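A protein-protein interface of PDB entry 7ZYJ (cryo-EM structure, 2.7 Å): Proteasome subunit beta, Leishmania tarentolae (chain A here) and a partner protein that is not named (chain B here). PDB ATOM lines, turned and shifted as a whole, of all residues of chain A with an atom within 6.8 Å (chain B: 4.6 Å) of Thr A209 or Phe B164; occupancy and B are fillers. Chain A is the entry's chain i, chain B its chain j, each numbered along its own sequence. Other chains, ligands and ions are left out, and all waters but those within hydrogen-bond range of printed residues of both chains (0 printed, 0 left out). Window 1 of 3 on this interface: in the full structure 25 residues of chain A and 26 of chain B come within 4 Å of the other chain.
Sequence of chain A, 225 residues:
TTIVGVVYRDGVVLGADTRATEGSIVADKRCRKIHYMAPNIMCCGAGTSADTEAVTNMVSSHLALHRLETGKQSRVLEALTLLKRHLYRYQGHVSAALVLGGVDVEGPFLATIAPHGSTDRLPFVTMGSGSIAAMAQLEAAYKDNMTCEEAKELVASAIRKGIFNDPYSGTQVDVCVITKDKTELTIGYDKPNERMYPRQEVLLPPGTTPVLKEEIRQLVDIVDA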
ATOM      1  N   LEU A 204      19.894  17.142 -14.710  1.00  0.00           N
ATOM      2  CA  LEU A 204      18.463  17.162 -15.009  1.00  0.00           C
ATOM      3  C   LEU A 204      18.301  17.232 -16.520  1.00  0.00           C
ATOM      4  O   LEU A 204      18.456  18.316 -17.113  1.00  0.00           O
ATOM      5  CB  LEU A 204      17.767  18.333 -14.326  1.00  0.00           C
ATOM      6  CG  LEU A 204      17.867  18.362 -12.800  1.00  0.00           C
ATOM      7  CD1 LEU A 204      17.245  19.629 -12.244  1.00  0.00           C
ATOM      8  CD2 LEU A 204      17.209  17.132 -12.198  1.00  0.00           C
ATOM      9  N   PRO A 205      18.012  16.112 -17.177  1.00  0.00           N
ATOM     10  CA  PRO A 205      17.914  16.102 -18.642  1.00  0.00           C
ATOM     11  C   PRO A 205      16.821  17.035 -19.128  1.00  0.00           C
ATOM     12  O   PRO A 205      15.781  17.182 -18.469  1.00  0.00           O
ATOM     13  CB  PRO A 205      17.582  14.637 -18.967  1.00  0.00           C
ATOM     14  CG  PRO A 205      17.072  14.056 -17.686  1.00  0.00           C
ATOM     15  CD  PRO A 205      17.790  14.779 -16.595  1.00  0.00           C
ATOM     16  N   PRO A 206      17.029  17.696 -20.267  1.00  0.00           N
ATOM     17  CA  PRO A 206      16.000  18.600 -20.805  1.00  0.00           C
ATOM     18  C   PRO A 206      14.694  17.863 -21.057  1.00  0.00           C
ATOM     19  O   PRO A 206      14.654  16.853 -21.764  1.00  0.00           O
ATOM     20  CB  PRO A 206      16.628  19.108 -22.108  1.00  0.00           C
ATOM     21  CG  PRO A 206      18.097  18.996 -21.879  1.00  0.00           C
ATOM     22  CD  PRO A 206      18.281  17.763 -21.039  1.00  0.00           C
ATOM     23  N   GLY A 207      13.619  18.379 -20.469  1.00  0.00           N
ATOM     24  CA  GLY A 207      12.306  17.767 -20.574  1.00  0.00           C
ATOM     25  C   GLY A 207      11.772  17.191 -19.279  1.00  0.00           C
ATOM     26  O   GLY A 207      10.659  16.646 -19.280  1.00  0.00           O
ATOM     27  N   THR A 208      12.507  17.279 -18.168  1.00  0.00           N
ATOM     28  CA  THR A 208      12.005  16.744 -16.907  1.00  0.00           C
ATOM     29  C   THR A 208      10.927  17.638 -16.304  1.00  0.00           C
ATOM     30  O   THR A 208      10.149  17.184 -15.458  1.00  0.00           O
ATOM     31  CB  THR A 208      13.154  16.553 -15.917  1.00  0.00           C
ATOM     32  OG1 THR A 208      12.655  15.965 -14.709  1.00  0.00           O
ATOM     33  CG2 THR A 208      13.814  17.885 -15.595  1.00  0.00           C
ATOM     34  N   THR A 209      10.866  18.903 -16.722  1.00  0.00           N
ATOM     35  CA  THR A 209       9.862  19.831 -16.225  1.00  0.00           C
ATOM     36  C   THR A 209       8.780  20.017 -17.274  1.00  0.00           C
ATOM     37  O   THR A 209       9.078  20.513 -18.371  1.00  0.00           O
ATOM     38  CB  THR A 209      10.494  21.174 -15.879  1.00  0.00           C
ATOM     39  OG1 THR A 209      11.245  21.655 -17.001  1.00  0.00           O
ATOM     40  CG2 THR A 209      11.421  21.032 -14.681  1.00  0.00           C
ATOM     41  N   PRO A 210       7.533  19.634 -16.999  1.00  0.00           N
ATOM     42  CA  PRO A 210       6.478  19.782 -18.009  1.00  0.00           C
ATOM     43  C   PRO A 210       6.221  21.243 -18.349  1.00  0.00           C
ATOM     44  O   PRO A 210       6.332  22.130 -17.500  1.00  0.00           O
ATOM     45  CB  PRO A 210       5.256  19.136 -17.344  1.00  0.00           C
ATOM     46  CG  PRO A 210       5.536  19.210 -15.882  1.00  0.00           C
ATOM     47  CD  PRO A 210       7.022  19.083 -15.732  1.00  0.00           C
ATOM     48  N   VAL A 211       5.870  21.481 -19.611  1.00  0.00           N
ATOM     49  CA  VAL A 211       5.653  22.819 -20.146  1.00  0.00           C
ATOM     50  C   VAL A 211       4.236  22.894 -20.697  1.00  0.00           C
ATOM     51  O   VAL A 211       3.776  21.969 -21.375  1.00  0.00           O
ATOM     52  CB  VAL A 211       6.692  23.165 -21.234  1.00  0.00           C
ATOM     53  CG1 VAL A 211       6.319  24.449 -21.955  1.00  0.00           C
ATOM     54  CG2 VAL A 211       8.080  23.276 -20.622  1.00  0.00           C
ATOM     55  N   GLU A 214       4.608  27.052 -25.071  1.00  0.00           N
ATOM     56  CA  GLU A 214       5.938  27.493 -25.458  1.00  0.00           C
ATOM     57  C   GLU A 214       5.830  28.452 -26.635  1.00  0.00           C
ATOM     58  O   GLU A 214       5.015  28.257 -27.540  1.00  0.00           O
ATOM     59  CB  GLU A 214       6.834  26.305 -25.837  1.00  0.00           C
ATOM     60  CG  GLU A 214       8.273  26.680 -26.143  1.00  0.00           C
ATOM     61  CD  GLU A 214       9.246  25.563 -25.828  1.00  0.00           C
ATOM     62  OE1 GLU A 214       8.987  24.799 -24.874  1.00  0.00           O
ATOM     63  OE2 GLU A 214      10.272  25.452 -26.530  1.00  0.00           O
ATOM     64  N   VAL B  21      18.204  32.692 -18.074  1.00  0.00           N
ATOM     65  CA  VAL B  21      16.817  32.285 -17.884  1.00  0.00           C
ATOM     66  C   VAL B  21      16.252  33.083 -16.722  1.00  0.00           C
ATOM     67  O   VAL B  21      16.798  33.044 -15.613  1.00  0.00           O
ATOM     68  CB  VAL B  21      16.693  30.776 -17.621  1.00  0.00           C
ATOM     69  CG1 VAL B  21      15.301  30.441 -17.113  1.00  0.00           C
ATOM     70  CG2 VAL B  21      17.005  29.990 -18.880  1.00  0.00           C
ATOM     71  N   PRO B 160      21.354  26.406 -22.616  1.00  0.00           N
ATOM     72  CA  PRO B 160      20.023  26.996 -22.382  1.00  0.00           C
ATOM     73  C   PRO B 160      18.987  26.004 -21.874  1.00  0.00           C
ATOM     74  O   PRO B 160      18.198  26.340 -20.982  1.00  0.00           O
ATOM     75  CB  PRO B 160      19.659  27.552 -23.763  1.00  0.00           C
ATOM     76  CG  PRO B 160      20.963  27.920 -24.363  1.00  0.00           C
ATOM     77  CD  PRO B 160      21.982  26.938 -23.839  1.00  0.00           C
ATOM     78  N   GLU B 161      18.980  24.779 -22.403  1.00  0.00           N
ATOM     79  CA  GLU B 161      18.009  23.789 -21.947  1.00  0.00           C
ATOM     80  C   GLU B 161      18.297  23.347 -20.518  1.00  0.00           C
ATOM     81  O   GLU B 161      17.385  23.286 -19.683  1.00  0.00           O
ATOM     82  CB  GLU B 161      18.005  22.587 -22.891  1.00  0.00           C
ATOM     83  CG  GLU B 161      17.633  22.926 -24.326  1.00  0.00           C
ATOM     84  CD  GLU B 161      16.231  23.488 -24.448  1.00  0.00           C
ATOM     85  OE1 GLU B 161      15.346  23.063 -23.676  1.00  0.00           O
ATOM     86  OE2 GLU B 161      16.012  24.356 -25.318  1.00  0.00           O
ATOM     87  N   GLU B 162      19.561  23.036 -20.219  1.00  0.00           N
ATOM     88  CA  GLU B 162      19.929  22.640 -18.865  1.00  0.00           C
ATOM     89  C   GLU B 162      19.676  23.770 -17.877  1.00  0.00           C
ATOM     90  O   GLU B 162      19.185  23.536 -16.764  1.00  0.00           O
ATOM     91  CB  GLU B 162      21.395  22.214 -18.834  1.00  0.00           C
ATOM     92  CG  GLU B 162      21.689  20.968 -19.650  1.00  0.00           C
ATOM     93  CD  GLU B 162      23.170  20.664 -19.737  1.00  0.00           C
ATOM     94  OE1 GLU B 162      23.979  21.524 -19.329  1.00  0.00           O
ATOM     95  OE2 GLU B 162      23.527  19.566 -20.214  1.00  0.00           O
ATOM     96  N   LEU B 163      20.003  25.002 -18.270  1.00  0.00           N
ATOM     97  CA  LEU B 163      19.751  26.150 -17.409  1.00  0.00           C
ATOM     98  C   LEU B 163      18.261  26.321 -17.149  1.00  0.00           C
ATOM     99  O   LEU B 163      17.850  26.612 -16.019  1.00  0.00           O
ATOM    100  CB  LEU B 163      20.331  27.414 -18.043  1.00  0.00           C
ATOM    101  CG  LEU B 163      20.457  28.628 -17.127  1.00  0.00           C
ATOM    102  CD1 LEU B 163      21.680  28.473 -16.244  1.00  0.00           C
ATOM    103  CD2 LEU B 163      20.526  29.909 -17.934  1.00  0.00           C
ATOM    104  N   PHE B 164      17.437  26.144 -18.184  1.00  0.00           N
ATOM    105  CA  PHE B 164      15.993  26.250 -18.007  1.00  0.00           C
ATOM    106  C   PHE B 164      15.476  25.183 -17.053  1.00  0.00           C
ATOM    107  O   PHE B 164      14.628  25.458 -16.198  1.00  0.00           O
ATOM    108  CB  PHE B 164      15.283  26.143 -19.355  1.00  0.00           C
ATOM    109  CG  PHE B 164      13.805  25.906 -19.237  1.00  0.00           C
ATOM    110  CD1 PHE B 164      12.945  26.947 -18.932  1.00  0.00           C
ATOM    111  CD2 PHE B 164      13.277  24.639 -19.418  1.00  0.00           C
ATOM    112  CE1 PHE B 164      11.587  26.730 -18.818  1.00  0.00           C
ATOM    113  CE2 PHE B 164      11.918  24.417 -19.302  1.00  0.00           C
ATOM    114  CZ  PHE B 164      11.073  25.464 -19.002  1.00  0.00           C
ATOM    115  N   GLU B 165      15.961  23.947 -17.200  1.00  0.00           N
ATOM    116  CA  GLU B 165      15.515  22.882 -16.305  1.00  0.00           C
ATOM    117  C   GLU B 165      15.910  23.172 -14.863  1.00  0.00           C
ATOM    118  O   GLU B 165      15.105  22.984 -13.939  1.00  0.00           O
ATOM    119  CB  GLU B 165      16.080  21.535 -16.755  1.00  0.00           C
ATOM    120  CG  GLU B 165      15.718  21.152 -18.179  1.00  0.00           C
ATOM    121  CD  GLU B 165      14.222  21.053 -18.397  1.00  0.00           C
ATOM    122  OE1 GLU B 165      13.514  20.589 -17.479  1.00  0.00           O
ATOM    123  OE2 GLU B 165      13.752  21.439 -19.488  1.00  0.00           O
ATOM    124  N   ILE B 166      17.141  23.642 -14.651  1.00  0.00           N
ATOM    125  CA  ILE B 166      17.587  23.976 -13.300  1.00  0.00           C
ATOM    126  C   ILE B 166      16.722  25.085 -12.716  1.00  0.00           C
ATOM    127  O   ILE B 166      16.283  25.013 -11.561  1.00  0.00           O
ATOM    128  CB  ILE B 166      19.076  24.368 -13.309  1.00  0.00           C
ATOM    129  CG1 ILE B 166      19.944  23.166 -13.682  1.00  0.00           C
ATOM    130  CG2 ILE B 166      19.491  24.925 -11.957  1.00  0.00           C
ATOM    131  CD1 ILE B 166      19.907  22.049 -12.671  1.00  0.00           C
ATOM    132  N   ALA B 167      16.462  26.127 -13.510  1.00  0.00           N
ATOM    133  CA  ALA B 167      15.658  27.244 -13.027  1.00  0.00           C
ATOM    134  C   ALA B 167      14.241  26.804 -12.689  1.00  0.00           C
ATOM    135  O   ALA B 167      13.688  27.207 -11.661  1.00  0.00           O
ATOM    136  CB  ALA B 167      15.638  28.364 -14.066  1.00  0.00           C
ATOM    137  N   ALA B 168      13.637  25.976 -13.543  1.00  0.00           N
ATOM    138  CA  ALA B 168      12.278  25.509 -13.294  1.00  0.00           C
ATOM    139  C   ALA B 168      12.208  24.665 -12.028  1.00  0.00           C
ATOM    140  O   ALA B 168      11.306  24.843 -11.197  1.00  0.00           O
ATOM    141  CB  ALA B 168      11.768  24.720 -14.499  1.00  0.00           C
ATOM    142  N   GLN B 169      13.155  23.737 -11.862  1.00  0.00           N
ATOM    143  CA  GLN B 169      13.165  22.904 -10.665  1.00  0.00           C
ATOM    144  C   GLN B 169      13.344  23.749  -9.412  1.00  0.00           C
ATOM    145  O   GLN B 169      12.631  23.565  -8.417  1.00  0.00           O
ATOM    146  CB  GLN B 169      14.266  21.849 -10.768  1.00  0.00           C
ATOM    147  CG  GLN B 169      13.837  20.581 -11.481  1.00  0.00           C
ATOM    148  CD  GLN B 169      12.580  19.980 -10.887  1.00  0.00           C
ATOM    149  OE1 GLN B 169      11.534  19.940 -11.532  1.00  0.00           O
ATOM    150  NE2 GLN B 169      12.677  19.511  -9.648  1.00  0.00           N
ATOM    151  N   ALA B 187       8.750  31.302 -17.654  1.00  0.00           N
ATOM    152  CA  ALA B 187      10.184  31.423 -17.841  1.00  0.00           C
ATOM    153  C   ALA B 187      10.494  32.017 -19.207  1.00  0.00           C
ATOM    154  O   ALA B 187       9.759  31.813 -20.179  1.00  0.00           O
ATOM    155  CB  ALA B 187      10.879  30.065 -17.696  1.00  0.00           C
ATOM    156  N   ILE B 189      13.885  32.286 -21.694  1.00  0.00           N
ATOM    157  CA  ILE B 189      15.257  31.923 -22.025  1.00  0.00           C
ATOM    158  C   ILE B 189      15.735  32.887 -23.099  1.00  0.00           C
ATOM    159  O   ILE B 189      15.189  32.911 -24.207  1.00  0.00           O
ATOM    160  CB  ILE B 189      15.351  30.470 -22.515  1.00  0.00           C
ATOM    161  CG1 ILE B 189      14.507  29.549 -21.634  1.00  0.00           C
ATOM    162  CG2 ILE B 189      16.799  30.011 -22.548  1.00  0.00           C
ATOM    163  CD1 ILE B 189      14.343  28.156 -22.201  1.00  0.00           C
ATOM    164  N   ARG B 198       8.239  30.185 -22.054  1.00  0.00           N
ATOM    165  CA  ARG B 198       7.648  28.909 -21.680  1.00  0.00           C
ATOM    166  C   ARG B 198       6.813  29.088 -20.423  1.00  0.00           C
ATOM    167  O   ARG B 198       7.097  29.964 -19.601  1.00  0.00           O
ATOM    168  CB  ARG B 198       8.727  27.844 -21.446  1.00  0.00           C
ATOM    169  CG  ARG B 198       9.479  27.441 -22.703  1.00  0.00           C
ATOM    170  CD  ARG B 198      10.536  26.388 -22.414  1.00  0.00           C
ATOM    171  NE  ARG B 198      11.269  26.022 -23.619  1.00  0.00           N
ATOM    172  CZ  ARG B 198      12.283  25.167 -23.654  1.00  0.00           C
ATOM    173  NH1 ARG B 198      12.711  24.558 -22.560  1.00  0.00           N
ATOM    174  NH2 ARG B 198      12.880  24.916 -24.815  1.00  0.00           N
ATOM    175  N   ILE B 200       5.389  26.821 -17.156  1.00  0.00           N
ATOM    176  CA  ILE B 200       5.824  25.612 -16.468  1.00  0.00           C
ATOM    177  C   ILE B 200       4.743  25.192 -15.483  1.00  0.00           C
ATOM    178  O   ILE B 200       4.279  26.005 -14.671  1.00  0.00           O
ATOM    179  CB  ILE B 200       7.166  25.828 -15.755  1.00  0.00           C
ATOM    180  CG1 ILE B 200       8.170  26.462 -16.717  1.00  0.00           C
ATOM    181  CG2 ILE B 200       7.701  24.514 -15.214  1.00  0.00           C
ATOM    182  CD1 ILE B 200       9.391  27.015 -16.042  1.00  0.00           C
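Of chain B, only Phe B164 (3.7 Å), Glu B165 (2.6 Å), Ala B168 (3.7 Å) and Gln B169 (3.3 Å) come within 4 Å of Thr A209.
Of chain A, only Thr A209 comes within 4 Å of Phe B164.
Printed residues of chain B within 4 Å of Leu A204: Ile B166 and Gln B169.
Printed residues of chain A within 4 Å of Ile B200: Pro A210 (3.6 Å).
Of the printed residues of chain B, Pro A206 touches Glu B161 (3.7 Å) and Glu B165 (3.7 Å).
Of the printed residues of chain A, Arg B198 touches Glu A214 (2.9 Å).
Ala B187 touches none of the printed residues of chain A.
The nearest residue of chain B that does not touch Thr A209 is Ile B200 (4.4 Å).
The nearest residue of chain A that does not touch Phe B164 is Val A211 (4.05 Å).
The nearest printed residue of chain B that does not touch Pro A205 is Glu B162 (6.2 Å).
Among the printed residues, pairs that only touch across the chains: Leu A204 with Ile B166 (3.6 Å), Leu A204 with Gln B169 (3.6 Å), Pro A205 with Glu B165 (3.98 Å), Pro A206 with Glu B161 (3.7 Å), Pro A206 with Glu B165 (3.7 Å), Thr A208 with Glu B165 (3.3 Å), Thr A209 with Phe B164 (3.7 Å), Thr A209 with Ala B168 (3.7 Å), Thr A209 with Gln B169 (3.3 Å) and Pro A210 with Ile B200 (3.6 Å).
Of the 15 printed residues of chain B, 8 touch a printed residue of chain A.
Hydrophobic or aromatic side chains of chain A within 4 Å of the printed part of chain B: Leu A204 and Pro A206.
Among the printed residues, 13 pairs touch across the chains.
The guanidinium group of Arg B198 is in salt-bridge range of the side-chain carboxylate of Glu B161, 3.2 Å away.
The backbone NH of Ala B187 is in hydrogen-bond range of the backbone carbonyl oxygen of Arg B198 (2.9 Å).
OE2 of Glu B165 lies within hydrogen-bond range of N of Gly A207, at 3.2 Å.
The side-chain carboxylate of Glu B165 is in hydrogen-bond range of the side-chain hydroxyl of Thr A209, at 2.6 Å.
The guanidinium group (NE) of Arg B198 is in salt-bridge range of the side-chain carboxylate (OE1) of Glu A214 (2.9 Å).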
